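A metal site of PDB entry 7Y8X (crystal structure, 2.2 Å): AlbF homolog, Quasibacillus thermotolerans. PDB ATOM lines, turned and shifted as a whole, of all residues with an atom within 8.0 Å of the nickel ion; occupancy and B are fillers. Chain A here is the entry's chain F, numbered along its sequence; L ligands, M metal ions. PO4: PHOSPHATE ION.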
ATOM      1  N   HIS A  54       2.266 -31.910 -10.770  1.00  0.00           N
ATOM      2  CA  HIS A  54       1.670 -31.195  -9.642  1.00  0.00           C
ATOM      3  C   HIS A  54       1.813 -32.004  -8.356  1.00  0.00           C
ATOM      4  O   HIS A  54       2.002 -31.432  -7.280  1.00  0.00           O
ATOM      5  CB  HIS A  54       0.202 -30.898  -9.928  1.00  0.00           C
ATOM      6  CG  HIS A  54      -0.512 -30.263  -8.784  1.00  0.00           C
ATOM      7  ND1 HIS A  54      -1.227 -30.997  -7.862  1.00  0.00           N
ATOM      8  CD2 HIS A  54      -0.607 -28.971  -8.390  1.00  0.00           C
ATOM      9  CE1 HIS A  54      -1.734 -30.187  -6.950  1.00  0.00           C
ATOM     10  NE2 HIS A  54      -1.375 -28.953  -7.247  1.00  0.00           N
ATOM     11  N   PHE A  55       1.699 -33.330  -8.447  1.00  0.00           N
ATOM     12  CA  PHE A  55       1.927 -34.167  -7.273  1.00  0.00           C
ATOM     13  C   PHE A  55       3.353 -33.985  -6.755  1.00  0.00           C
ATOM     14  O   PHE A  55       3.573 -33.805  -5.559  1.00  0.00           O
ATOM     15  CB  PHE A  55       1.662 -35.633  -7.618  1.00  0.00           C
ATOM     16  CG  PHE A  55       1.376 -36.507  -6.414  1.00  0.00           C
ATOM     17  CD1 PHE A  55       2.348 -36.710  -5.440  1.00  0.00           C
ATOM     18  CD2 PHE A  55       0.150 -37.131  -6.269  1.00  0.00           C
ATOM     19  CE1 PHE A  55       2.093 -37.509  -4.346  1.00  0.00           C
ATOM     20  CE2 PHE A  55      -0.111 -37.931  -5.167  1.00  0.00           C
ATOM     21  CZ  PHE A  55       0.858 -38.116  -4.207  1.00  0.00           C
ATOM     22  N   GLU A  57       5.293 -31.440  -7.148  1.00  0.00           N
ATOM     23  CA  GLU A  57       5.386 -30.113  -6.555  1.00  0.00           C
ATOM     24  C   GLU A  57       5.002 -30.137  -5.081  1.00  0.00           C
ATOM     25  O   GLU A  57       5.653 -29.485  -4.251  1.00  0.00           O
ATOM     26  CB  GLU A  57       4.495 -29.126  -7.316  1.00  0.00           C
ATOM     27  CG  GLU A  57       4.399 -27.761  -6.663  1.00  0.00           C
ATOM     28  CD  GLU A  57       3.143 -27.014  -7.067  1.00  0.00           C
ATOM     29  OE1 GLU A  57       2.778 -27.034  -8.261  1.00  0.00           O
ATOM     30  OE2 GLU A  57       2.511 -26.408  -6.178  1.00  0.00           O
ATOM     31  N   HIS A  58       3.943 -30.867  -4.741  1.00  0.00           N
ATOM     32  CA  HIS A  58       3.546 -30.992  -3.336  1.00  0.00           C
ATOM     33  C   HIS A  58       4.570 -31.793  -2.546  1.00  0.00           C
ATOM     34  O   HIS A  58       4.868 -31.457  -1.393  1.00  0.00           O
ATOM     35  CB  HIS A  58       2.167 -31.628  -3.234  1.00  0.00           C
ATOM     36  CG  HIS A  58       1.038 -30.664  -3.396  1.00  0.00           C
ATOM     37  ND1 HIS A  58      -0.015 -30.598  -2.508  1.00  0.00           N
ATOM     38  CD2 HIS A  58       0.811 -29.714  -4.332  1.00  0.00           C
ATOM     39  CE1 HIS A  58      -0.849 -29.648  -2.899  1.00  0.00           C
ATOM     40  NE2 HIS A  58      -0.368 -29.094  -3.990  1.00  0.00           N
ATOM     41  N   ALA A  81       4.699 -21.923  -4.900  1.00  0.00           N
ATOM     42  CA  ALA A  81       4.952 -22.918  -5.934  1.00  0.00           C
ATOM     43  C   ALA A  81       3.697 -23.132  -6.754  1.00  0.00           C
ATOM     44  O   ALA A  81       2.573 -23.041  -6.246  1.00  0.00           O
ATOM     45  CB  ALA A  81       5.419 -24.254  -5.337  1.00  0.00           C
ATOM     46  N   TYR A  82       3.891 -23.407  -8.043  1.00  0.00           N
ATOM     47  CA  TYR A  82       2.783 -23.695  -8.932  1.00  0.00           C
ATOM     48  C   TYR A  82       3.296 -24.470 -10.140  1.00  0.00           C
ATOM     49  O   TYR A  82       4.443 -24.315 -10.547  1.00  0.00           O
ATOM     50  CB  TYR A  82       2.066 -22.409  -9.383  1.00  0.00           C
ATOM     51  CG  TYR A  82       2.982 -21.349  -9.961  1.00  0.00           C
ATOM     52  CD1 TYR A  82       3.640 -20.458  -9.131  1.00  0.00           C
ATOM     53  CD2 TYR A  82       3.170 -21.251 -11.326  1.00  0.00           C
ATOM     54  CE1 TYR A  82       4.471 -19.484  -9.654  1.00  0.00           C
ATOM     55  CE2 TYR A  82       4.001 -20.282 -11.862  1.00  0.00           C
ATOM     56  CZ  TYR A  82       4.651 -19.400 -11.014  1.00  0.00           C
ATOM     57  OH  TYR A  82       5.483 -18.426 -11.536  1.00  0.00           O
ATOM     58  N   THR A  83       2.425 -25.301 -10.699  1.00  0.00           N
ATOM     59  CA  THR A  83       2.739 -26.106 -11.861  1.00  0.00           C
ATOM     60  C   THR A  83       1.943 -25.589 -13.054  1.00  0.00           C
ATOM     61  O   THR A  83       0.728 -25.424 -12.966  1.00  0.00           O
ATOM     62  CB  THR A  83       2.414 -27.585 -11.607  1.00  0.00           C
ATOM     63  OG1 THR A  83       3.217 -28.080 -10.534  1.00  0.00           O
ATOM     64  CG2 THR A  83       2.668 -28.415 -12.855  1.00  0.00           C
ATOM     65  N   GLU A 123      -0.091 -36.422   0.786  1.00  0.00           N
ATOM     66  CA  GLU A 123      -0.233 -35.431  -0.271  1.00  0.00           C
ATOM     67  C   GLU A 123      -1.270 -35.848  -1.305  1.00  0.00           C
ATOM     68  O   GLU A 123      -1.927 -34.987  -1.896  1.00  0.00           O
ATOM     69  CB  GLU A 123       1.117 -35.171  -0.931  1.00  0.00           C
ATOM     70  CG  GLU A 123       2.100 -34.397  -0.049  1.00  0.00           C
ATOM     71  CD  GLU A 123       1.577 -33.030   0.363  1.00  0.00           C
ATOM     72  OE1 GLU A 123       0.745 -32.455  -0.385  1.00  0.00           O
ATOM     73  OE2 GLU A 123       1.995 -32.532   1.420  1.00  0.00           O
ATOM     74  N   ILE A 126      -4.497 -34.690   0.094  1.00  0.00           N
ATOM     75  CA  ILE A 126      -4.587 -33.238  -0.040  1.00  0.00           C
ATOM     76  C   ILE A 126      -4.958 -32.869  -1.473  1.00  0.00           C
ATOM     77  O   ILE A 126      -5.814 -32.006  -1.698  1.00  0.00           O
ATOM     78  CB  ILE A 126      -3.263 -32.587   0.387  1.00  0.00           C
ATOM     79  CG1 ILE A 126      -3.048 -32.743   1.894  1.00  0.00           C
ATOM     80  CG2 ILE A 126      -3.239 -31.111   0.002  1.00  0.00           C
ATOM     81  CD1 ILE A 126      -1.712 -32.198   2.372  1.00  0.00           C
ATOM     82  N   ILE A 127      -4.330 -33.508  -2.455  1.00  0.00           N
ATOM     83  CA  ILE A 127      -4.583 -33.171  -3.852  1.00  0.00           C
ATOM     84  C   ILE A 127      -5.968 -33.608  -4.283  1.00  0.00           C
ATOM     85  O   ILE A 127      -6.624 -32.920  -5.076  1.00  0.00           O
ATOM     86  CB  ILE A 127      -3.478 -33.775  -4.742  1.00  0.00           C
ATOM     87  CG1 ILE A 127      -2.133 -33.113  -4.425  1.00  0.00           C
ATOM     88  CG2 ILE A 127      -3.816 -33.614  -6.217  1.00  0.00           C
ATOM     89  CD1 ILE A 127      -0.965 -33.741  -5.130  1.00  0.00           C
ATOM     90  N   GLU A 130      -8.235 -30.985  -3.409  1.00  0.00           N
ATOM     91  CA  GLU A 130      -8.148 -29.892  -4.382  1.00  0.00           C
ATOM     92  C   GLU A 130      -8.949 -30.208  -5.631  1.00  0.00           C
ATOM     93  O   GLU A 130      -9.626 -29.323  -6.184  1.00  0.00           O
ATOM     94  CB  GLU A 130      -6.680 -29.626  -4.748  1.00  0.00           C
ATOM     95  CG  GLU A 130      -5.955 -28.736  -3.778  1.00  0.00           C
ATOM     96  CD  GLU A 130      -4.507 -28.526  -4.176  1.00  0.00           C
ATOM     97  OE1 GLU A 130      -3.829 -29.516  -4.514  1.00  0.00           O
ATOM     98  OE2 GLU A 130      -4.049 -27.365  -4.174  1.00  0.00           O
ATOM     99  N   ARG A 149      -6.527 -26.113 -15.157  1.00  0.00           N
ATOM    100  CA  ARG A 149      -6.237 -26.447 -13.771  1.00  0.00           C
ATOM    101  C   ARG A 149      -6.493 -27.926 -13.489  1.00  0.00           C
ATOM    102  O   ARG A 149      -5.657 -28.610 -12.898  1.00  0.00           O
ATOM    103  CB  ARG A 149      -7.055 -25.568 -12.827  1.00  0.00           C
ATOM    104  CG  ARG A 149      -6.837 -25.900 -11.357  1.00  0.00           C
ATOM    105  CD  ARG A 149      -7.558 -24.920 -10.444  1.00  0.00           C
ATOM    106  NE  ARG A 149      -7.231 -25.159  -9.047  1.00  0.00           N
ATOM    107  CZ  ARG A 149      -6.149 -24.696  -8.443  1.00  0.00           C
ATOM    108  NH1 ARG A 149      -5.257 -23.950  -9.076  1.00  0.00           N
ATOM    109  NH2 ARG A 149      -5.945 -24.990  -7.158  1.00  0.00           N
ATOM    110  N   ILE A 152      -3.818 -30.054 -14.908  1.00  0.00           N
ATOM    111  CA  ILE A 152      -2.593 -30.041 -14.115  1.00  0.00           C
ATOM    112  C   ILE A 152      -2.779 -30.864 -12.843  1.00  0.00           C
ATOM    113  O   ILE A 152      -1.909 -31.657 -12.462  1.00  0.00           O
ATOM    114  CB  ILE A 152      -2.160 -28.593 -13.807  1.00  0.00           C
ATOM    115  CG1 ILE A 152      -1.713 -27.899 -15.103  1.00  0.00           C
ATOM    116  CG2 ILE A 152      -1.056 -28.574 -12.765  1.00  0.00           C
ATOM    117  CD1 ILE A 152      -1.567 -26.398 -14.962  1.00  0.00           C
ATOM    118  N   LEU A 153      -3.910 -30.682 -12.157  1.00  0.00           N
ATOM    119  CA  LEU A 153      -4.200 -31.466 -10.961  1.00  0.00           C
ATOM    120  C   LEU A 153      -4.408 -32.940 -11.275  1.00  0.00           C
ATOM    121  O   LEU A 153      -4.227 -33.778 -10.392  1.00  0.00           O
ATOM    122  CB  LEU A 153      -5.445 -30.923 -10.247  1.00  0.00           C
ATOM    123  CG  LEU A 153      -5.474 -29.457  -9.826  1.00  0.00           C
ATOM    124  CD1 LEU A 153      -6.760 -29.139  -9.084  1.00  0.00           C
ATOM    125  CD2 LEU A 153      -4.262 -29.104  -8.978  1.00  0.00           C
HETATM  126  P   PO4 L   1      -0.748 -25.345  -5.950  1.00  0.00           P
HETATM  127  O1  PO4 L   1      -2.254 -25.394  -6.078  1.00  0.00           O
HETATM  128  O2  PO4 L   1      -0.129 -25.893  -7.211  1.00  0.00           O
HETATM  129  O3  PO4 L   1      -0.308 -26.177  -4.779  1.00  0.00           O
HETATM  130  O4  PO4 L   1      -0.304 -23.915  -5.750  1.00  0.00           O
HETATM  131 NI    NI M   1      -1.804 -27.549  -5.406  1.00  0.00          NI
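The side-chain carboxylate (OE1) of Glu 123 sits at hydrogen-bond distance from a ring nitrogen (ND1) of His 58, 2.9 Å away.
The nearest printed residue that does not touch the nickel ion is Glu 57 (4.5 Å).
The nickel ion is bound by an oxygen (O3) of the ligand (2.1 Å), an oxygen (O1) of the ligand (2.3 Å), a ring nitrogen (NE2) of His 54 (2.4 Å), a ring nitrogen (NE2) of His 58 (2.5 Å) and the side-chain carboxylate of Glu 130 (2.6 Å).
The nickel ion has five donor atoms within binding distance.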
